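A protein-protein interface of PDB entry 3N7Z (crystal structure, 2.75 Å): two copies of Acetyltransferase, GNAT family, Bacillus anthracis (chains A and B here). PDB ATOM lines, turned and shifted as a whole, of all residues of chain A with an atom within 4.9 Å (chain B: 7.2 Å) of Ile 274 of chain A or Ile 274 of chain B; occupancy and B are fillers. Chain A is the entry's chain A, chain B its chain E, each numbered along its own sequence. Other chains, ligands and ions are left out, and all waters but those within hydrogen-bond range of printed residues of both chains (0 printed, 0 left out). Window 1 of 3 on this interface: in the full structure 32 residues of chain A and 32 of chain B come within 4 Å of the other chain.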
ATOM      1  N   LEU A 134      20.522  -5.181   8.723  1.00  0.00           N
ATOM      2  CA  LEU A 134      19.720  -4.096   9.243  1.00  0.00           C
ATOM      3  C   LEU A 134      20.120  -2.793   8.563  1.00  0.00           C
ATOM      4  O   LEU A 134      21.304  -2.556   8.284  1.00  0.00           O
ATOM      5  CB  LEU A 134      19.877  -3.973  10.748  1.00  0.00           C
ATOM      6  CG  LEU A 134      19.266  -5.088  11.583  1.00  0.00           C
ATOM      7  CD1 LEU A 134      19.716  -4.928  13.020  1.00  0.00           C
ATOM      8  CD2 LEU A 134      17.743  -5.065  11.487  1.00  0.00           C
ATOM      9  N   LEU A 135      19.110  -1.973   8.274  1.00  0.00           N
ATOM     10  CA  LEU A 135      19.303  -0.624   7.770  1.00  0.00           C
ATOM     11  C   LEU A 135      18.985   0.352   8.888  1.00  0.00           C
ATOM     12  O   LEU A 135      17.868   0.381   9.389  1.00  0.00           O
ATOM     13  CB  LEU A 135      18.396  -0.364   6.564  1.00  0.00           C
ATOM     14  CG  LEU A 135      18.562   0.977   5.841  1.00  0.00           C
ATOM     15  CD1 LEU A 135      18.145   0.835   4.400  1.00  0.00           C
ATOM     16  CD2 LEU A 135      17.764   2.100   6.516  1.00  0.00           C
ATOM     17  N   GLU A 257      15.778  -3.188   4.307  1.00  0.00           N
ATOM     18  CA  GLU A 257      16.161  -2.518   3.061  1.00  0.00           C
ATOM     19  C   GLU A 257      14.955  -2.414   2.125  1.00  0.00           C
ATOM     20  O   GLU A 257      15.025  -1.764   1.088  1.00  0.00           O
ATOM     21  CB  GLU A 257      17.299  -3.277   2.358  1.00  0.00           C
ATOM     22  CG  GLU A 257      18.239  -4.087   3.279  1.00  0.00           C
ATOM     23  CD  GLU A 257      19.330  -4.871   2.525  1.00  0.00           C
ATOM     24  OE1 GLU A 257      19.928  -4.334   1.564  1.00  0.00           O
ATOM     25  OE2 GLU A 257      19.606  -6.027   2.917  1.00  0.00           O
ATOM     26  N   VAL A 270      19.701  11.172   3.351  1.00  0.00           N
ATOM     27  CA  VAL A 270      20.019  11.129   4.764  1.00  0.00           C
ATOM     28  C   VAL A 270      21.044  10.029   4.974  1.00  0.00           C
ATOM     29  O   VAL A 270      21.317   9.254   4.061  1.00  0.00           O
ATOM     30  CB  VAL A 270      18.769  10.867   5.619  1.00  0.00           C
ATOM     31  CG1 VAL A 270      17.776  12.000   5.456  1.00  0.00           C
ATOM     32  CG2 VAL A 270      18.128   9.535   5.243  1.00  0.00           C
ATOM     33  N   THR A 272      22.273   6.613   5.894  1.00  0.00           N
ATOM     34  CA  THR A 272      21.582   5.337   5.739  1.00  0.00           C
ATOM     35  C   THR A 272      22.618   4.244   5.580  1.00  0.00           C
ATOM     36  O   THR A 272      23.335   4.205   4.582  1.00  0.00           O
ATOM     37  CB  THR A 272      20.705   5.323   4.477  1.00  0.00           C
ATOM     38  OG1 THR A 272      19.837   6.452   4.485  1.00  0.00           O
ATOM     39  CG2 THR A 272      19.860   4.072   4.413  1.00  0.00           C
ATOM     40  N   GLU A 273      22.677   3.342   6.552  1.00  0.00           N
ATOM     41  CA  GLU A 273      23.727   2.331   6.583  1.00  0.00           C
ATOM     42  C   GLU A 273      23.177   0.923   6.663  1.00  0.00           C
ATOM     43  O   GLU A 273      22.348   0.628   7.517  1.00  0.00           O
ATOM     44  CB  GLU A 273      24.677   2.596   7.746  1.00  0.00           C
ATOM     45  CG  GLU A 273      23.994   3.234   8.941  1.00  0.00           C
ATOM     46  CD  GLU A 273      24.928   3.453  10.108  1.00  0.00           C
ATOM     47  OE1 GLU A 273      26.150   3.631   9.861  1.00  0.00           O
ATOM     48  OE2 GLU A 273      24.435   3.448  11.267  1.00  0.00           O
ATOM     49  N   ILE A 274      23.638   0.074   5.751  1.00  0.00           N
ATOM     50  CA  ILE A 274      23.280  -1.335   5.745  1.00  0.00           C
ATOM     51  C   ILE A 274      24.347  -2.152   6.453  1.00  0.00           C
ATOM     52  O   ILE A 274      25.436  -2.349   5.930  1.00  0.00           O
ATOM     53  CB  ILE A 274      23.042  -1.902   4.312  1.00  0.00           C
ATOM     54  CG1 ILE A 274      24.011  -1.290   3.296  1.00  0.00           C
ATOM     55  CG2 ILE A 274      21.645  -1.611   3.855  1.00  0.00           C
ATOM     56  CD1 ILE A 274      24.433  -2.257   2.172  1.00  0.00           C
ATOM     57  N   LYS A 275      24.032  -2.611   7.658  1.00  0.00           N
ATOM     58  CA  LYS A 275      24.923  -3.504   8.391  1.00  0.00           C
ATOM     59  C   LYS A 275      24.467  -4.968   8.342  1.00  0.00           C
ATOM     60  O   LYS A 275      23.370  -5.294   8.784  1.00  0.00           O
ATOM     61  CB  LYS A 275      25.094  -3.038   9.843  1.00  0.00           C
ATOM     62  CG  LYS A 275      23.788  -2.589  10.549  1.00  0.00           C
ATOM     63  CD  LYS A 275      24.062  -1.971  11.938  1.00  0.00           C
ATOM     64  CE  LYS A 275      24.929  -0.704  11.833  1.00  0.00           C
ATOM     65  NZ  LYS A 275      25.317  -0.195  13.180  1.00  0.00           N
ATOM     66  N   PRO A 276      25.305  -5.853   7.781  1.00  0.00           N
ATOM     67  CA  PRO A 276      25.081  -7.269   7.983  1.00  0.00           C
ATOM     68  C   PRO A 276      24.865  -7.532   9.464  1.00  0.00           C
ATOM     69  O   PRO A 276      25.612  -7.016  10.300  1.00  0.00           O
ATOM     70  CB  PRO A 276      26.394  -7.888   7.509  1.00  0.00           C
ATOM     71  CG  PRO A 276      26.838  -6.980   6.445  1.00  0.00           C
ATOM     72  CD  PRO A 276      26.443  -5.607   6.881  1.00  0.00           C
ATOM     73  N   ASN B 133      22.030   5.488  -6.755  1.00  0.00           N
ATOM     74  CA  ASN B 133      22.822   5.649  -5.537  1.00  0.00           C
ATOM     75  C   ASN B 133      24.321   5.397  -5.755  1.00  0.00           C
ATOM     76  O   ASN B 133      24.749   4.819  -6.773  1.00  0.00           O
ATOM     77  CB  ASN B 133      22.348   4.723  -4.402  1.00  0.00           C
ATOM     78  CG  ASN B 133      20.854   4.663  -4.260  1.00  0.00           C
ATOM     79  OD1 ASN B 133      20.185   5.666  -4.081  1.00  0.00           O
ATOM     80  ND2 ASN B 133      20.324   3.466  -4.311  1.00  0.00           N
ATOM     81  N   LEU B 134      25.103   5.837  -4.768  1.00  0.00           N
ATOM     82  CA  LEU B 134      26.467   5.383  -4.567  1.00  0.00           C
ATOM     83  C   LEU B 134      26.506   4.698  -3.232  1.00  0.00           C
ATOM     84  O   LEU B 134      25.843   5.139  -2.277  1.00  0.00           O
ATOM     85  CB  LEU B 134      27.449   6.547  -4.513  1.00  0.00           C
ATOM     86  CG  LEU B 134      27.646   7.448  -5.718  1.00  0.00           C
ATOM     87  CD1 LEU B 134      28.395   8.668  -5.241  1.00  0.00           C
ATOM     88  CD2 LEU B 134      28.383   6.744  -6.857  1.00  0.00           C
ATOM     89  N   LEU B 135      27.287   3.625  -3.169  1.00  0.00           N
ATOM     90  CA  LEU B 135      27.587   2.948  -1.912  1.00  0.00           C
ATOM     91  C   LEU B 135      28.989   3.358  -1.471  1.00  0.00           C
ATOM     92  O   LEU B 135      29.960   3.201  -2.212  1.00  0.00           O
ATOM     93  CB  LEU B 135      27.509   1.431  -2.100  1.00  0.00           C
ATOM     94  CG  LEU B 135      27.474   0.493  -0.880  1.00  0.00           C
ATOM     95  CD1 LEU B 135      26.061   0.383  -0.347  1.00  0.00           C
ATOM     96  CD2 LEU B 135      27.999  -0.907  -1.247  1.00  0.00           C
ATOM     97  N   VAL B 136      29.093   3.923  -0.281  1.00  0.00           N
ATOM     98  CA  VAL B 136      30.395   4.256   0.249  1.00  0.00           C
ATOM     99  C   VAL B 136      30.670   3.361   1.440  1.00  0.00           C
ATOM    100  O   VAL B 136      29.918   3.353   2.418  1.00  0.00           O
ATOM    101  CB  VAL B 136      30.503   5.734   0.665  1.00  0.00           C
ATOM    102  CG1 VAL B 136      31.935   6.057   1.117  1.00  0.00           C
ATOM    103  CG2 VAL B 136      30.053   6.666  -0.487  1.00  0.00           C
ATOM    104  N   GLU B 257      25.721  -0.836  -5.731  1.00  0.00           N
ATOM    105  CA  GLU B 257      25.071  -1.802  -4.845  1.00  0.00           C
ATOM    106  C   GLU B 257      25.300  -3.247  -5.337  1.00  0.00           C
ATOM    107  O   GLU B 257      25.414  -4.166  -4.529  1.00  0.00           O
ATOM    108  CB  GLU B 257      23.588  -1.450  -4.672  1.00  0.00           C
ATOM    109  CG  GLU B 257      23.398   0.045  -4.313  1.00  0.00           C
ATOM    110  CD  GLU B 257      21.948   0.452  -3.990  1.00  0.00           C
ATOM    111  OE1 GLU B 257      21.477   0.157  -2.857  1.00  0.00           O
ATOM    112  OE2 GLU B 257      21.299   1.097  -4.858  1.00  0.00           O
ATOM    113  N   LEU B 262      32.431  -6.844  -0.255  1.00  0.00           N
ATOM    114  CA  LEU B 262      32.379  -6.861   1.211  1.00  0.00           C
ATOM    115  C   LEU B 262      32.099  -8.249   1.773  1.00  0.00           C
ATOM    116  O   LEU B 262      32.725  -8.680   2.753  1.00  0.00           O
ATOM    117  CB  LEU B 262      31.308  -5.904   1.714  1.00  0.00           C
ATOM    118  CG  LEU B 262      31.669  -4.442   1.942  1.00  0.00           C
ATOM    119  CD1 LEU B 262      32.586  -3.894   0.857  1.00  0.00           C
ATOM    120  CD2 LEU B 262      30.368  -3.641   2.040  1.00  0.00           C
ATOM    121  N   PRO B 268      32.776  -9.073   7.441  1.00  0.00           N
ATOM    122  CA  PRO B 268      31.915  -8.342   6.509  1.00  0.00           C
ATOM    123  C   PRO B 268      31.078  -7.219   7.137  1.00  0.00           C
ATOM    124  O   PRO B 268      30.583  -6.359   6.405  1.00  0.00           O
ATOM    125  CB  PRO B 268      30.989  -9.436   5.958  1.00  0.00           C
ATOM    126  CG  PRO B 268      31.683 -10.710   6.225  1.00  0.00           C
ATOM    127  CD  PRO B 268      32.387 -10.492   7.514  1.00  0.00           C
ATOM    128  N   ARG B 269      30.910  -7.228   8.460  1.00  0.00           N
ATOM    129  CA  ARG B 269      30.201  -6.146   9.146  1.00  0.00           C
ATOM    130  C   ARG B 269      31.079  -4.921   9.222  1.00  0.00           C
ATOM    131  O   ARG B 269      31.625  -4.589  10.272  1.00  0.00           O
ATOM    132  CB  ARG B 269      29.819  -6.548  10.558  1.00  0.00           C
ATOM    133  CG  ARG B 269      28.673  -7.498  10.648  1.00  0.00           C
ATOM    134  CD  ARG B 269      28.524  -7.965  12.078  1.00  0.00           C
ATOM    135  NE  ARG B 269      29.667  -8.764  12.502  1.00  0.00           N
ATOM    136  CZ  ARG B 269      29.728  -9.449  13.634  1.00  0.00           C
ATOM    137  NH1 ARG B 269      28.708  -9.444  14.479  1.00  0.00           N
ATOM    138  NH2 ARG B 269      30.814 -10.147  13.917  1.00  0.00           N
ATOM    139  N   VAL B 270      31.229  -4.249   8.098  1.00  0.00           N
ATOM    140  CA  VAL B 270      31.941  -2.983   8.082  1.00  0.00           C
ATOM    141  C   VAL B 270      30.951  -1.833   7.812  1.00  0.00           C
ATOM    142  O   VAL B 270      29.811  -2.085   7.377  1.00  0.00           O
ATOM    143  CB  VAL B 270      33.118  -3.014   7.088  1.00  0.00           C
ATOM    144  CG1 VAL B 270      34.097  -4.049   7.523  1.00  0.00           C
ATOM    145  CG2 VAL B 270      32.645  -3.312   5.662  1.00  0.00           C
ATOM    146  N   LYS B 271      31.381  -0.598   8.099  1.00  0.00           N
ATOM    147  CA  LYS B 271      30.598   0.622   7.815  1.00  0.00           C
ATOM    148  C   LYS B 271      30.326   0.846   6.303  1.00  0.00           C
ATOM    149  O   LYS B 271      31.253   1.037   5.514  1.00  0.00           O
ATOM    150  CB  LYS B 271      31.291   1.843   8.439  1.00  0.00           C
ATOM    151  CG  LYS B 271      30.403   3.080   8.530  1.00  0.00           C
ATOM    152  CD  LYS B 271      30.694   3.902   9.804  1.00  0.00           C
ATOM    153  CE  LYS B 271      29.528   4.865  10.157  1.00  0.00           C
ATOM    154  NZ  LYS B 271      29.284   5.919   9.116  1.00  0.00           N
ATOM    155  N   THR B 272      29.045   0.823   5.927  1.00  0.00           N
ATOM    156  CA  THR B 272      28.609   0.874   4.518  1.00  0.00           C
ATOM    157  C   THR B 272      27.384   1.757   4.351  1.00  0.00           C
ATOM    158  O   THR B 272      26.301   1.401   4.810  1.00  0.00           O
ATOM    159  CB  THR B 272      28.216  -0.536   4.011  1.00  0.00           C
ATOM    160  OG1 THR B 272      29.331  -1.421   4.149  1.00  0.00           O
ATOM    161  CG2 THR B 272      27.776  -0.507   2.557  1.00  0.00           C
ATOM    162  N   GLU B 273      27.537   2.889   3.676  1.00  0.00           N
ATOM    163  CA  GLU B 273      26.409   3.821   3.511  1.00  0.00           C
ATOM    164  C   GLU B 273      25.904   3.904   2.069  1.00  0.00           C
ATOM    165  O   GLU B 273      26.698   3.996   1.136  1.00  0.00           O
ATOM    166  CB  GLU B 273      26.752   5.208   4.076  1.00  0.00           C
ATOM    167  CG  GLU B 273      28.173   5.658   3.738  1.00  0.00           C
ATOM    168  CD  GLU B 273      28.699   6.807   4.604  1.00  0.00           C
ATOM    169  OE1 GLU B 273      28.058   7.891   4.607  1.00  0.00           O
ATOM    170  OE2 GLU B 273      29.767   6.623   5.250  1.00  0.00           O
ATOM    171  N   ILE B 274      24.581   3.827   1.913  1.00  0.00           N
ATOM    172  CA  ILE B 274      23.888   4.063   0.644  1.00  0.00           C
ATOM    173  C   ILE B 274      23.432   5.510   0.577  1.00  0.00           C
ATOM    174  O   ILE B 274      22.554   5.936   1.327  1.00  0.00           O
ATOM    175  CB  ILE B 274      22.675   3.115   0.436  1.00  0.00           C
ATOM    176  CG1 ILE B 274      22.018   2.767   1.781  1.00  0.00           C
ATOM    177  CG2 ILE B 274      23.104   1.853  -0.283  1.00  0.00           C
ATOM    178  CD1 ILE B 274      21.050   1.548   1.778  1.00  0.00           C
ATOM    179  N   LYS B 275      24.062   6.277  -0.307  1.00  0.00           N
ATOM    180  CA  LYS B 275      23.677   7.677  -0.527  1.00  0.00           C
ATOM    181  C   LYS B 275      22.967   7.805  -1.867  1.00  0.00           C
ATOM    182  O   LYS B 275      23.568   7.528  -2.904  1.00  0.00           O
ATOM    183  CB  LYS B 275      24.900   8.615  -0.546  1.00  0.00           C
ATOM    184  CG  LYS B 275      26.244   7.975  -0.208  1.00  0.00           C
ATOM    185  CD  LYS B 275      27.359   9.011  -0.125  1.00  0.00           C
ATOM    186  CE  LYS B 275      27.461   9.606   1.267  1.00  0.00           C
ATOM    187  NZ  LYS B 275      28.397  10.756   1.276  1.00  0.00           N
ATOM    188  N   PRO B 276      21.686   8.212  -1.854  1.00  0.00           N
ATOM    189  CA  PRO B 276      21.087   8.639  -3.111  1.00  0.00           C
ATOM    190  C   PRO B 276      21.989   9.710  -3.697  1.00  0.00           C
ATOM    191  O   PRO B 276      22.520  10.534  -2.955  1.00  0.00           O
ATOM    192  CB  PRO B 276      19.748   9.233  -2.680  1.00  0.00           C
ATOM    193  CG  PRO B 276      19.427   8.547  -1.421  1.00  0.00           C
ATOM    194  CD  PRO B 276      20.723   8.246  -0.741  1.00  0.00           C
ATOM    195  N   TYR B 277      22.180   9.689  -5.007  1.00  0.00           N
ATOM    196  CA  TYR B 277      23.246  10.476  -5.598  1.00  0.00           C
ATOM    197  C   TYR B 277      22.761  11.426  -6.685  1.00  0.00           C
ATOM    198  O   TYR B 277      22.904  12.651  -6.568  1.00  0.00           O
ATOM    199  CB  TYR B 277      24.348   9.544  -6.120  1.00  0.00           C
ATOM    200  CG  TYR B 277      25.493  10.227  -6.837  1.00  0.00           C
ATOM    201  CD1 TYR B 277      26.100  11.356  -6.303  1.00  0.00           C
ATOM    202  CD2 TYR B 277      25.981   9.727  -8.037  1.00  0.00           C
ATOM    203  CE1 TYR B 277      27.157  11.981  -6.952  1.00  0.00           C
ATOM    204  CE2 TYR B 277      27.036  10.344  -8.700  1.00  0.00           C
ATOM    205  CZ  TYR B 277      27.622  11.473  -8.152  1.00  0.00           C
ATOM    206  OH  TYR B 277      28.672  12.097  -8.787  1.00  0.00           O
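OE1 of Glu 273 of chain A lies within salt-bridge range of NZ of Lys 271 of chain B, at 3.95 Å. The backbone NH of Ile 274 of chain B lies within hydrogen-bond range of the backbone carbonyl oxygen of Thr 272 of chain A, 3.0 Å away. N of Ile 274 of chain A lies within hydrogen-bond range of O of Thr 272 of chain B.
O of Val 270 of chain B is in hydrogen-bond range of OG1 of Thr 272 of chain B, at 3.3 Å. The side-chain carboxylate of Glu 273 of chain B is in salt-bridge range of the side-chain amino group of Lys 271 of chain B (3.96 Å). The backbone carbonyl oxygen of Val 136 of chain B sits at hydrogen-bond distance from the backbone NH of Glu 273 of chain B, at 2.7 Å. The backbone carbonyl oxygen of Val 270 of chain A lies within hydrogen-bond range of the side-chain hydroxyl of Thr 272 of chain A, at 3.2 Å.
Ile 274 of chain B touches Leu 135 of chain A. O of Thr 272 of chain A touches CA of Glu 273 of chain B, at 3.3 Å. Thr 272 of chain B touches Glu 273 of chain A. Ile 274 of chain A touches Leu 135 of chain B. Ile 274 of chain B touches Ile 274 of chain A. CG of Pro 276 of chain A touches O of Pro 268 of chain B (3.8 Å). Pro 276 of chain A touches Arg 269 of chain B.
Of the printed residues of chain B, Leu 135 of chain A touches Ile 274 (3.98 Å). Val 270 of chain A touches none of the printed residues of chain B. Of the printed residues of chain B, Thr 272 of chain A touches Glu 273 (3.3 Å) and Ile 274 (3.0 Å). Printed residues of chain B within 4 Å of Ile 274 of chain A: Leu 135 (3.996 Å), Thr 272 (3.1 Å) and Ile 274 (3.8 Å). Asn 133 of chain B touches none of the printed residues of chain A. Ile 274 of chain B touches just these residues of chain A: Leu 135, Thr 272 and Ile 274. The nearest residue of chain A that does not touch Ile 274 of chain B is Val 270 of chain A (4.5 Å).
Printed residues of chain A that touch a printed residue of chain B: Leu 135, Thr 272, Glu 273, Ile 274 and Pro 276. Hydrophobic or aromatic side chains of chain A that line the printed part of chain B: Leu 135, Ile 274 and Pro 276. Along chain B the printed residues that touch a printed residue of chain A span positions 135 to 274. Among the printed residues, Asp or Glu carboxylates within 4 Å of a Lys or Arg side-chain nitrogen of the other chain: Glu 273 of chain A with Lys 271 of chain B.
Leu 135 of chain A touches Ile 274 of chain B, and with the chains exchanged Ile 274 of chain A touches Leu 135 of chain B. Thr 272 of chain A touches Glu 273 of chain B, and with the chains exchanged Glu 273 of chain A touches Thr 272 of chain B. Thr 272 of chain A touches Ile 274 of chain B, and with the chains exchanged Ile 274 of chain A touches Thr 272 of chain B. Ile 274 of chain B touches its own counterpart, Ile 274 of chain A. Of the 10 pairs that touch across the chains among the printed residues, 7 have their exchanged pair printed and touching as well.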
